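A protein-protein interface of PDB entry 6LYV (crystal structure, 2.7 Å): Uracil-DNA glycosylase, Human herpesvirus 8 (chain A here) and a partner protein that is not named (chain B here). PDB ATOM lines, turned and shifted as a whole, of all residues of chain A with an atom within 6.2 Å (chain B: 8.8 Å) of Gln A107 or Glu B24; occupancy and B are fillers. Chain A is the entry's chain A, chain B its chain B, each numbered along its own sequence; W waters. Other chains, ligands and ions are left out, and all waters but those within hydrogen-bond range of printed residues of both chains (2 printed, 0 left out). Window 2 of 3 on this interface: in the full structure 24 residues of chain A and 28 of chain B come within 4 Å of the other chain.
Hydrophobic or aromatic side chains of chain A that line the printed part of chain B: Pro A109.
Hydrophobic or aromatic side chains of chain B that line the printed part of chain A: Tyr B57 and His B62.
Among the printed residues, 9 pairs touch across the chains.
Among the printed residues, no Asp or Glu carboxylate lies within 4 Å of a Lys or Arg side-chain nitrogen of the other chain.
Of the printed residues of chain B, Gln A107 touches Glu B24 (3.8 Å), Tyr B57 (3.9 Å), Ser B58 (3.1 Å) and Asp B59 (3.4 Å).
Printed residues of chain B within 4 Å of Pro A109: Glu B26 (3.2 Å) and Tyr B57 (3.97 Å).
Printed residues of chain B within 4 Å of Arg A113: His B62 (3.4 Å).
Glu B4 touches none of the printed residues of chain A.
Glu B24 touches just one residue of chain A: Gln A107.
Printed residues of chain A within 4 Å of Cys B25: Gln A94.
Thr B55 touches none of the printed residues of chain A.
Printed residues of chain A within 4 Å of Tyr B57: Gln A94 (2.9 Å), Gln A107 (3.9 Å) and Pro A109 (3.97 Å).
Of the printed residues of chain A, Ser B58 touches Gln A107.
The backbone NH (N) of Lys A92 lies within hydrogen-bond range of the side-chain amide oxygen (OE1) of Gln A94, 3.0 Å away.
The backbone carbonyl oxygen (O) of Val A108 lies within hydrogen-bond range of the guanidinium group (NH1) of Arg A113 (3.2 Å).
OE1 of Glu B21 lies within hydrogen-bond range of OG of Ser B58, 2.8 Å away.
OE2 of Glu B21 sits at hydrogen-bond distance from N of Asp B59 (3.1 Å).
O of Glu B24 sits at hydrogen-bond distance from N of Tyr B57 (2.9 Å).
O of Thr B55 is in hydrogen-bond range of N of Glu B26.
Water W1 lies within hydrogen-bond range of the side-chain amide nitrogen of Gln A107 (2.7 Å) and the backbone NH of Asp B59 (3.1 Å).
Water W2 lies within hydrogen-bond range of OH of Tyr B57 (2.8 Å), O of Gln A107 (2.8 Å) and OE1 of Glu B24 (3.0 Å).
The side-chain amide nitrogen of Gln A94 lies within hydrogen-bond range of the backbone carbonyl oxygen of Cys B25.
The side-chain hydroxyl of Tyr B57 is in hydrogen-bond range of the side-chain amide nitrogen of Gln A94 (2.9 Å).
The side-chain amide oxygen (OE1) of Gln A107 sits close to the backbone carbonyl oxygen (O) of Ser B58 (3.4 Å).
OE1 of Gln A107 lies within hydrogen-bond range of N of Asp B59, at 3.4 Å.
A ring nitrogen (ND1) of His B62 lies close to the guanidinium group (NH2) of Arg A113 (3.4 Å).
Gln A107 touches Glu B24 (NE2 to OE1, 3.8 Å).
CB of Gln A107 touches CE2 of Tyr B57, at 3.9 Å.
OE1 of Glu B26 touches CB of Pro A109 (3.2 Å).
Pro A109 touches Tyr B57.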
ATOM      1  N   LYS A  92     -19.249   8.338 -21.040  1.00  0.00           N
ATOM      2  CA  LYS A  92     -18.622   9.497 -20.416  1.00  0.00           C
ATOM      3  C   LYS A  92     -17.331   9.900 -21.122  1.00  0.00           C
ATOM      4  O   LYS A  92     -16.447  10.504 -20.507  1.00  0.00           O
ATOM      5  CB  LYS A  92     -18.356   9.234 -18.934  1.00  0.00           C
ATOM      6  CG  LYS A  92     -19.627   9.028 -18.117  1.00  0.00           C
ATOM      7  CD  LYS A  92     -20.493  10.286 -18.082  1.00  0.00           C
ATOM      8  CE  LYS A  92     -19.841  11.407 -17.295  1.00  0.00           C
ATOM      9  NZ  LYS A  92     -19.799  11.079 -15.847  1.00  0.00           N
ATOM     10  N   GLN A  94     -15.009   7.854 -22.681  1.00  0.00           N
ATOM     11  CA  GLN A  94     -13.929   6.881 -22.760  1.00  0.00           C
ATOM     12  C   GLN A  94     -13.944   6.079 -24.054  1.00  0.00           C
ATOM     13  O   GLN A  94     -12.925   5.472 -24.399  1.00  0.00           O
ATOM     14  CB  GLN A  94     -13.991   5.920 -21.570  1.00  0.00           C
ATOM     15  CG  GLN A  94     -14.264   6.584 -20.229  1.00  0.00           C
ATOM     16  CD  GLN A  94     -15.735   6.555 -19.844  1.00  0.00           C
ATOM     17  OE1 GLN A  94     -16.599   6.975 -20.613  1.00  0.00           O
ATOM     18  NE2 GLN A  94     -16.024   6.058 -18.648  1.00  0.00           N
ATOM     19  N   VAL A 102     -10.211   1.820 -24.140  1.00  0.00           N
ATOM     20  CA  VAL A 102     -10.218   3.230 -23.778  1.00  0.00           C
ATOM     21  C   VAL A 102      -8.943   3.874 -24.306  1.00  0.00           C
ATOM     22  O   VAL A 102      -7.990   3.198 -24.695  1.00  0.00           O
ATOM     23  CB  VAL A 102     -10.353   3.455 -22.257  1.00  0.00           C
ATOM     24  CG1 VAL A 102     -11.706   2.978 -21.777  1.00  0.00           C
ATOM     25  CG2 VAL A 102      -9.233   2.748 -21.508  1.00  0.00           C
ATOM     26  N   ASP A 103      -8.950   5.204 -24.334  1.00  0.00           N
ATOM     27  CA  ASP A 103      -7.801   5.952 -24.819  1.00  0.00           C
ATOM     28  C   ASP A 103      -6.588   5.733 -23.913  1.00  0.00           C
ATOM     29  O   ASP A 103      -6.734   5.450 -22.721  1.00  0.00           O
ATOM     30  CB  ASP A 103      -8.142   7.437 -24.896  1.00  0.00           C
ATOM     31  CG  ASP A 103      -8.932   7.781 -26.137  1.00  0.00           C
ATOM     32  OD1 ASP A 103      -8.824   7.029 -27.131  1.00  0.00           O
ATOM     33  OD2 ASP A 103      -9.660   8.798 -26.119  1.00  0.00           O
ATOM     34  N   GLN A 105      -4.754   7.746 -22.463  1.00  0.00           N
ATOM     35  CA  GLN A 105      -4.716   8.687 -21.350  1.00  0.00           C
ATOM     36  C   GLN A 105      -5.717   8.363 -20.249  1.00  0.00           C
ATOM     37  O   GLN A 105      -5.587   8.892 -19.139  1.00  0.00           O
ATOM     38  CB  GLN A 105      -4.953  10.115 -21.852  1.00  0.00           C
ATOM     39  CG  GLN A 105      -3.873  10.626 -22.791  1.00  0.00           C
ATOM     40  CD  GLN A 105      -2.510  10.701 -22.122  1.00  0.00           C
ATOM     41  OE1 GLN A 105      -1.613   9.909 -22.416  1.00  0.00           O
ATOM     42  NE2 GLN A 105      -2.353  11.658 -21.213  1.00  0.00           N
ATOM     43  N   CYS A 106      -6.705   7.518 -20.523  1.00  0.00           N
ATOM     44  CA  CYS A 106      -7.783   7.271 -19.580  1.00  0.00           C
ATOM     45  C   CYS A 106      -7.445   6.117 -18.639  1.00  0.00           C
ATOM     46  O   CYS A 106      -6.632   5.244 -18.947  1.00  0.00           O
ATOM     47  CB  CYS A 106      -9.083   6.966 -20.327  1.00  0.00           C
ATOM     48  SG  CYS A 106      -9.706   8.339 -21.320  1.00  0.00           S
ATOM     49  N   GLN A 107      -8.091   6.130 -17.475  1.00  0.00           N
ATOM     50  CA  GLN A 107      -7.995   5.017 -16.543  1.00  0.00           C
ATOM     51  C   GLN A 107      -8.612   3.764 -17.144  1.00  0.00           C
ATOM     52  O   GLN A 107      -9.500   3.829 -17.998  1.00  0.00           O
ATOM     53  CB  GLN A 107      -8.716   5.338 -15.238  1.00  0.00           C
ATOM     54  CG  GLN A 107      -8.060   6.377 -14.377  1.00  0.00           C
ATOM     55  CD  GLN A 107      -8.776   6.528 -13.049  1.00  0.00           C
ATOM     56  OE1 GLN A 107      -8.874   5.573 -12.273  1.00  0.00           O
ATOM     57  NE2 GLN A 107      -9.297   7.725 -12.788  1.00  0.00           N
ATOM     58  N   VAL A 108      -8.133   2.612 -16.688  1.00  0.00           N
ATOM     59  CA  VAL A 108      -8.685   1.334 -17.122  1.00  0.00           C
ATOM     60  C   VAL A 108      -9.998   1.101 -16.385  1.00  0.00           C
ATOM     61  O   VAL A 108     -10.016   1.058 -15.146  1.00  0.00           O
ATOM     62  CB  VAL A 108      -7.687   0.193 -16.883  1.00  0.00           C
ATOM     63  CG1 VAL A 108      -8.296  -1.141 -17.292  1.00  0.00           C
ATOM     64  CG2 VAL A 108      -6.398   0.462 -17.647  1.00  0.00           C
ATOM     65  N   PRO A 109     -11.114   0.964 -17.092  1.00  0.00           N
ATOM     66  CA  PRO A 109     -12.408   0.761 -16.425  1.00  0.00           C
ATOM     67  C   PRO A 109     -12.463  -0.595 -15.742  1.00  0.00           C
ATOM     68  O   PRO A 109     -11.614  -1.461 -16.002  1.00  0.00           O
ATOM     69  CB  PRO A 109     -13.419   0.857 -17.580  1.00  0.00           C
ATOM     70  CG  PRO A 109     -12.698   1.583 -18.666  1.00  0.00           C
ATOM     71  CD  PRO A 109     -11.263   1.172 -18.540  1.00  0.00           C
ATOM     72  N   ARG A 113     -10.299  -3.868 -16.540  1.00  0.00           N
ATOM     73  CA  ARG A 113      -9.354  -4.251 -15.493  1.00  0.00           C
ATOM     74  C   ARG A 113      -9.476  -5.731 -15.161  1.00  0.00           C
ATOM     75  O   ARG A 113      -8.466  -6.427 -14.985  1.00  0.00           O
ATOM     76  CB  ARG A 113      -9.592  -3.397 -14.240  1.00  0.00           C
ATOM     77  CG  ARG A 113      -8.345  -3.092 -13.392  1.00  0.00           C
ATOM     78  CD  ARG A 113      -8.314  -1.643 -12.879  1.00  0.00           C
ATOM     79  NE  ARG A 113      -7.084  -0.938 -13.252  1.00  0.00           N
ATOM     80  CZ  ARG A 113      -6.924   0.382 -13.177  1.00  0.00           C
ATOM     81  NH1 ARG A 113      -7.928   1.144 -12.766  1.00  0.00           N
ATOM     82  NH2 ARG A 113      -5.768   0.943 -13.521  1.00  0.00           N
ATOM     83  N   GLY A 132      -5.479   1.177 -21.331  1.00  0.00           N
ATOM     84  CA  GLY A 132      -6.536   0.301 -21.793  1.00  0.00           C
ATOM     85  C   GLY A 132      -6.834   0.372 -23.276  1.00  0.00           C
ATOM     86  O   GLY A 132      -7.934   0.011 -23.704  1.00  0.00           O
ATOM     87  N   GLU B   4     -25.274  10.043  -7.868  1.00  0.00           N
ATOM     88  CA  GLU B   4     -23.844   9.773  -7.986  1.00  0.00           C
ATOM     89  C   GLU B   4     -23.050  10.540  -6.936  1.00  0.00           C
ATOM     90  O   GLU B   4     -22.148   9.982  -6.302  1.00  0.00           O
ATOM     91  CB  GLU B   4     -23.344  10.122  -9.387  1.00  0.00           C
ATOM     92  CG  GLU B   4     -24.017   9.348 -10.500  1.00  0.00           C
ATOM     93  CD  GLU B   4     -23.245   9.426 -11.805  1.00  0.00           C
ATOM     94  OE1 GLU B   4     -22.480  10.402 -11.979  1.00  0.00           O
ATOM     95  OE2 GLU B   4     -23.391   8.503 -12.643  1.00  0.00           O
ATOM     96  N   LYS B   8     -20.821   9.117  -3.890  1.00  0.00           N
ATOM     97  CA  LYS B   8     -19.430   9.534  -3.747  1.00  0.00           C
ATOM     98  C   LYS B   8     -19.160  10.095  -2.357  1.00  0.00           C
ATOM     99  O   LYS B   8     -18.159   9.751  -1.720  1.00  0.00           O
ATOM    100  CB  LYS B   8     -19.086  10.563  -4.822  1.00  0.00           C
ATOM    101  CG  LYS B   8     -17.661  11.067  -4.754  1.00  0.00           C
ATOM    102  CD  LYS B   8     -17.326  11.877  -5.986  1.00  0.00           C
ATOM    103  CE  LYS B   8     -15.980  12.546  -5.849  1.00  0.00           C
ATOM    104  NZ  LYS B   8     -15.687  13.395  -7.036  1.00  0.00           N
ATOM    105  N   GLU B  21     -11.393  14.069  -5.561  1.00  0.00           N
ATOM    106  CA  GLU B  21     -10.949  13.199  -6.644  1.00  0.00           C
ATOM    107  C   GLU B  21     -12.073  12.936  -7.639  1.00  0.00           C
ATOM    108  O   GLU B  21     -13.222  12.704  -7.257  1.00  0.00           O
ATOM    109  CB  GLU B  21     -10.435  11.875  -6.084  1.00  0.00           C
ATOM    110  CG  GLU B  21      -9.858  10.951  -7.140  1.00  0.00           C
ATOM    111  CD  GLU B  21      -9.538   9.575  -6.596  1.00  0.00           C
ATOM    112  OE1 GLU B  21     -10.291   9.098  -5.718  1.00  0.00           O
ATOM    113  OE2 GLU B  21      -8.543   8.969  -7.047  1.00  0.00           O
ATOM    114  N   LYS B  22     -11.733  12.959  -8.927  1.00  0.00           N
ATOM    115  CA  LYS B  22     -12.721  12.738  -9.973  1.00  0.00           C
ATOM    116  C   LYS B  22     -13.071  11.261 -10.082  1.00  0.00           C
ATOM    117  O   LYS B  22     -12.184  10.405 -10.149  1.00  0.00           O
ATOM    118  CB  LYS B  22     -12.213  13.243 -11.321  1.00  0.00           C
ATOM    119  CG  LYS B  22     -13.216  13.006 -12.443  1.00  0.00           C
ATOM    120  CD  LYS B  22     -12.717  13.466 -13.799  1.00  0.00           C
ATOM    121  CE  LYS B  22     -13.723  13.099 -14.883  1.00  0.00           C
ATOM    122  NZ  LYS B  22     -13.275  13.507 -16.243  1.00  0.00           N
ATOM    123  N   TRP B  23     -14.367  10.968 -10.109  1.00  0.00           N
ATOM    124  CA  TRP B  23     -14.867   9.620 -10.334  1.00  0.00           C
ATOM    125  C   TRP B  23     -15.311   9.466 -11.783  1.00  0.00           C
ATOM    126  O   TRP B  23     -15.918  10.373 -12.358  1.00  0.00           O
ATOM    127  CB  TRP B  23     -16.039   9.309  -9.402  1.00  0.00           C
ATOM    128  CG  TRP B  23     -15.637   8.930  -8.011  1.00  0.00           C
ATOM    129  CD1 TRP B  23     -14.454   9.212  -7.391  1.00  0.00           C
ATOM    130  CD2 TRP B  23     -16.423   8.202  -7.060  1.00  0.00           C
ATOM    131  NE1 TRP B  23     -14.455   8.706  -6.116  1.00  0.00           N
ATOM    132  CE2 TRP B  23     -15.653   8.081  -5.888  1.00  0.00           C
ATOM    133  CE3 TRP B  23     -17.704   7.643  -7.087  1.00  0.00           C
ATOM    134  CZ2 TRP B  23     -16.118   7.419  -4.755  1.00  0.00           C
ATOM    135  CZ3 TRP B  23     -18.166   6.985  -5.961  1.00  0.00           C
ATOM    136  CH2 TRP B  23     -17.374   6.879  -4.811  1.00  0.00           C
ATOM    137  N   GLU B  24     -15.007   8.314 -12.367  1.00  0.00           N
ATOM    138  CA  GLU B  24     -15.516   7.944 -13.677  1.00  0.00           C
ATOM    139  C   GLU B  24     -16.446   6.748 -13.532  1.00  0.00           C
ATOM    140  O   GLU B  24     -16.424   6.039 -12.522  1.00  0.00           O
ATOM    141  CB  GLU B  24     -14.380   7.640 -14.663  1.00  0.00           C
ATOM    142  CG  GLU B  24     -13.665   8.889 -15.176  1.00  0.00           C
ATOM    143  CD  GLU B  24     -12.560   8.579 -16.176  1.00  0.00           C
ATOM    144  OE1 GLU B  24     -11.636   7.806 -15.839  1.00  0.00           O
ATOM    145  OE2 GLU B  24     -12.621   9.108 -17.309  1.00  0.00           O
ATOM    146  N   CYS B  25     -17.293   6.545 -14.539  1.00  0.00           N
ATOM    147  CA  CYS B  25     -18.371   5.571 -14.443  1.00  0.00           C
ATOM    148  C   CYS B  25     -18.373   4.637 -15.642  1.00  0.00           C
ATOM    149  O   CYS B  25     -18.266   5.084 -16.787  1.00  0.00           O
ATOM    150  CB  CYS B  25     -19.726   6.270 -14.336  1.00  0.00           C
ATOM    151  SG  CYS B  25     -21.120   5.131 -14.244  1.00  0.00           S
ATOM    152  N   GLU B  26     -18.504   3.343 -15.371  1.00  0.00           N
ATOM    153  CA  GLU B  26     -18.717   2.328 -16.393  1.00  0.00           C
ATOM    154  C   GLU B  26     -20.114   1.750 -16.215  1.00  0.00           C
ATOM    155  O   GLU B  26     -20.474   1.322 -15.114  1.00  0.00           O
ATOM    156  CB  GLU B  26     -17.672   1.214 -16.298  1.00  0.00           C
ATOM    157  CG  GLU B  26     -17.988   0.019 -17.174  1.00  0.00           C
ATOM    158  CD  GLU B  26     -17.098  -1.171 -16.885  1.00  0.00           C
ATOM    159  OE1 GLU B  26     -15.893  -1.117 -17.198  1.00  0.00           O
ATOM    160  OE2 GLU B  26     -17.607  -2.167 -16.339  1.00  0.00           O
ATOM    161  N   SER B  27     -20.901   1.748 -17.287  1.00  0.00           N
ATOM    162  CA  SER B  27     -22.276   1.272 -17.236  1.00  0.00           C
ATOM    163  C   SER B  27     -22.410  -0.021 -18.028  1.00  0.00           C
ATOM    164  O   SER B  27     -21.974  -0.098 -19.181  1.00  0.00           O
ATOM    165  CB  SER B  27     -23.244   2.327 -17.771  1.00  0.00           C
ATOM    166  OG  SER B  27     -24.585   1.920 -17.568  1.00  0.00           O
ATOM    167  N   TYR B  54     -24.143   0.759 -12.785  1.00  0.00           N
ATOM    168  CA  TYR B  54     -23.158   1.827 -12.894  1.00  0.00           C
ATOM    169  C   TYR B  54     -22.052   1.567 -11.883  1.00  0.00           C
ATOM    170  O   TYR B  54     -22.300   1.583 -10.677  1.00  0.00           O
ATOM    171  CB  TYR B  54     -23.800   3.197 -12.656  1.00  0.00           C
ATOM    172  CG  TYR B  54     -24.932   3.515 -13.610  1.00  0.00           C
ATOM    173  CD1 TYR B  54     -24.689   4.136 -14.827  1.00  0.00           C
ATOM    174  CD2 TYR B  54     -26.244   3.193 -13.290  1.00  0.00           C
ATOM    175  CE1 TYR B  54     -25.723   4.426 -15.701  1.00  0.00           C
ATOM    176  CE2 TYR B  54     -27.280   3.478 -14.155  1.00  0.00           C
ATOM    177  CZ  TYR B  54     -27.017   4.093 -15.359  1.00  0.00           C
ATOM    178  OH  TYR B  54     -28.052   4.377 -16.219  1.00  0.00           O
ATOM    179  N   THR B  55     -20.841   1.320 -12.372  1.00  0.00           N
ATOM    180  CA  THR B  55     -19.681   1.070 -11.525  1.00  0.00           C
ATOM    181  C   THR B  55     -18.713   2.240 -11.634  1.00  0.00           C
ATOM    182  O   THR B  55     -18.324   2.632 -12.739  1.00  0.00           O
ATOM    183  CB  THR B  55     -18.983  -0.231 -11.923  1.00  0.00           C
ATOM    184  OG1 THR B  55     -19.946  -1.290 -11.975  1.00  0.00           O
ATOM    185  CG2 THR B  55     -17.897  -0.585 -10.917  1.00  0.00           C
ATOM    186  N   TYR B  56     -18.309   2.778 -10.489  1.00  0.00           N
ATOM    187  CA  TYR B  56     -17.488   3.976 -10.431  1.00  0.00           C
ATOM    188  C   TYR B  56     -16.058   3.598 -10.073  1.00  0.00           C
ATOM    189  O   TYR B  56     -15.827   2.655  -9.310  1.00  0.00           O
ATOM    190  CB  TYR B  56     -18.060   4.977  -9.424  1.00  0.00           C
ATOM    191  CG  TYR B  56     -19.486   5.351  -9.750  1.00  0.00           C
ATOM    192  CD1 TYR B  56     -19.770   6.386 -10.628  1.00  0.00           C
ATOM    193  CD2 TYR B  56     -20.550   4.642  -9.212  1.00  0.00           C
ATOM    194  CE1 TYR B  56     -21.070   6.716 -10.947  1.00  0.00           C
ATOM    195  CE2 TYR B  56     -21.852   4.965  -9.526  1.00  0.00           C
ATOM    196  CZ  TYR B  56     -22.106   6.004 -10.394  1.00  0.00           C
ATOM    197  OH  TYR B  56     -23.407   6.328 -10.708  1.00  0.00           O
ATOM    198  N   TYR B  57     -15.103   4.314 -10.655  1.00  0.00           N
ATOM    199  CA  TYR B  57     -13.700   3.965 -10.505  1.00  0.00           C
ATOM    200  C   TYR B  57     -12.855   5.232 -10.502  1.00  0.00           C
ATOM    201  O   TYR B  57     -13.218   6.242 -11.110  1.00  0.00           O
ATOM    202  CB  TYR B  57     -13.246   3.008 -11.613  1.00  0.00           C
ATOM    203  CG  TYR B  57     -13.433   3.530 -13.022  1.00  0.00           C
ATOM    204  CD1 TYR B  57     -14.679   3.509 -13.631  1.00  0.00           C
ATOM    205  CD2 TYR B  57     -12.358   4.016 -13.753  1.00  0.00           C
ATOM    206  CE1 TYR B  57     -14.855   3.974 -14.922  1.00  0.00           C
ATOM    207  CE2 TYR B  57     -12.523   4.483 -15.046  1.00  0.00           C
ATOM    208  CZ  TYR B  57     -13.774   4.458 -15.625  1.00  0.00           C
ATOM    209  OH  TYR B  57     -13.948   4.922 -16.909  1.00  0.00           O
ATOM    210  N   SER B  58     -11.727   5.162  -9.801  1.00  0.00           N
ATOM    211  CA  SER B  58     -10.771   6.259  -9.733  1.00  0.00           C
ATOM    212  C   SER B  58      -9.437   5.691  -9.268  1.00  0.00           C
ATOM    213  O   SER B  58      -9.281   4.479  -9.100  1.00  0.00           O
ATOM    214  CB  SER B  58     -11.264   7.378  -8.810  1.00  0.00           C
ATOM    215  OG  SER B  58     -11.111   7.026  -7.448  1.00  0.00           O
ATOM    216  N   ASP B  59      -8.461   6.581  -9.073  1.00  0.00           N
ATOM    217  CA  ASP B  59      -7.140   6.140  -8.635  1.00  0.00           C
ATOM    218  C   ASP B  59      -7.185   5.599  -7.209  1.00  0.00           C
ATOM    219  O   ASP B  59      -6.738   4.477  -6.945  1.00  0.00           O
ATOM    220  CB  ASP B  59      -6.144   7.295  -8.741  1.00  0.00           C
ATOM    221  CG  ASP B  59      -5.580   7.451 -10.138  1.00  0.00           C
ATOM    222  OD1 ASP B  59      -5.488   6.437 -10.863  1.00  0.00           O
ATOM    223  OD2 ASP B  59      -5.227   8.589 -10.513  1.00  0.00           O
ATOM    224  N   THR B  60      -7.724   6.386  -6.273  1.00  0.00           N
ATOM    225  CA  THR B  60      -7.811   5.924  -4.891  1.00  0.00           C
ATOM    226  C   THR B  60      -8.813   4.788  -4.743  1.00  0.00           C
ATOM    227  O   THR B  60      -8.647   3.927  -3.870  1.00  0.00           O
ATOM    228  CB  THR B  60      -8.178   7.082  -3.960  1.00  0.00           C
ATOM    229  OG1 THR B  60      -9.497   7.545  -4.267  1.00  0.00           O
ATOM    230  CG2 THR B  60      -7.195   8.231  -4.128  1.00  0.00           C
ATOM    231  N   LEU B  61      -9.860   4.770  -5.572  1.00  0.00           N
ATOM    232  CA  LEU B  61     -10.779   3.637  -5.567  1.00  0.00           C
ATOM    233  C   LEU B  61     -10.072   2.368  -6.019  1.00  0.00           C
ATOM    234  O   LEU B  61     -10.354   1.275  -5.513  1.00  0.00           O
ATOM    235  CB  LEU B  61     -11.989   3.928  -6.455  1.00  0.00           C
ATOM    236  CG  LEU B  61     -13.019   4.920  -5.911  1.00  0.00           C
ATOM    237  CD1 LEU B  61     -14.092   5.200  -6.947  1.00  0.00           C
ATOM    238  CD2 LEU B  61     -13.640   4.400  -4.627  1.00  0.00           C
ATOM    239  N   HIS B  62      -9.150   2.494  -6.975  1.00  0.00           N
ATOM    240  CA  HIS B  62      -8.354   1.348  -7.399  1.00  0.00           C
ATOM    241  C   HIS B  62      -7.399   0.905  -6.293  1.00  0.00           C
ATOM    242  O   HIS B  62      -7.300  -0.290  -5.987  1.00  0.00           O
ATOM    243  CB  HIS B  62      -7.599   1.705  -8.683  1.00  0.00           C
ATOM    244  CG  HIS B  62      -6.714   0.614  -9.200  1.00  0.00           C
ATOM    245  ND1 HIS B  62      -5.680   0.856 -10.079  1.00  0.00           N
ATOM    246  CD2 HIS B  62      -6.712  -0.721  -8.977  1.00  0.00           C
ATOM    247  CE1 HIS B  62      -5.073  -0.282 -10.366  1.00  0.00           C
ATOM    248  NE2 HIS B  62      -5.680  -1.254  -9.711  1.00  0.00           N
ATOM    249  N   GLU B  63      -6.704   1.858  -5.661  1.00  0.00           N
ATOM    250  CA  GLU B  63      -5.800   1.508  -4.566  1.00  0.00           C
ATOM    251  C   GLU B  63      -6.537   0.891  -3.385  1.00  0.00           C
ATOM    252  O   GLU B  63      -5.963   0.071  -2.659  1.00  0.00           O
ATOM    253  CB  GLU B  63      -5.003   2.734  -4.112  1.00  0.00           C
ATOM    254  CG  GLU B  63      -3.899   3.153  -5.073  1.00  0.00           C
ATOM    255  CD  GLU B  63      -2.810   2.095  -5.198  1.00  0.00           C
ATOM    256  OE1 GLU B  63      -2.543   1.390  -4.198  1.00  0.00           O
ATOM    257  OE2 GLU B  63      -2.224   1.962  -6.295  1.00  0.00           O
ATOM    258  N   TYR B  67     -15.265  -0.915  -5.444  1.00  0.00           N
ATOM    259  CA  TYR B  67     -16.057  -0.607  -6.634  1.00  0.00           C
ATOM    260  C   TYR B  67     -17.427  -0.108  -6.197  1.00  0.00           C
ATOM    261  O   TYR B  67     -18.350  -0.910  -5.985  1.00  0.00           O
ATOM    262  CB  TYR B  67     -16.192  -1.827  -7.542  1.00  0.00           C
ATOM    263  CG  TYR B  67     -14.897  -2.279  -8.171  1.00  0.00           C
ATOM    264  CD1 TYR B  67     -14.399  -1.646  -9.302  1.00  0.00           C
ATOM    265  CD2 TYR B  67     -14.179  -3.347  -7.644  1.00  0.00           C
ATOM    266  CE1 TYR B  67     -13.218  -2.055  -9.888  1.00  0.00           C
ATOM    267  CE2 TYR B  67     -12.996  -3.767  -8.225  1.00  0.00           C
ATOM    268  CZ  TYR B  67     -12.522  -3.117  -9.346  1.00  0.00           C
ATOM    269  OH  TYR B  67     -11.347  -3.524  -9.931  1.00  0.00           O
ATOM    270  N   PRO B  68     -17.603   1.201  -6.038  1.00  0.00           N
ATOM    271  CA  PRO B  68     -18.944   1.729  -5.765  1.00  0.00           C
ATOM    272  C   PRO B  68     -19.846   1.526  -6.968  1.00  0.00           C
ATOM    273  O   PRO B  68     -19.401   1.600  -8.116  1.00  0.00           O
ATOM    274  CB  PRO B  68     -18.699   3.218  -5.491  1.00  0.00           C
ATOM    275  CG  PRO B  68     -17.231   3.325  -5.191  1.00  0.00           C
ATOM    276  CD  PRO B  68     -16.575   2.251  -6.005  1.00  0.00           C
HETATM  277  O   HOH W   1      -8.584   9.190 -10.696  1.00  0.00           O
HETATM  278  O   HOH W   2     -11.570   5.767 -18.028  1.00  0.00           O
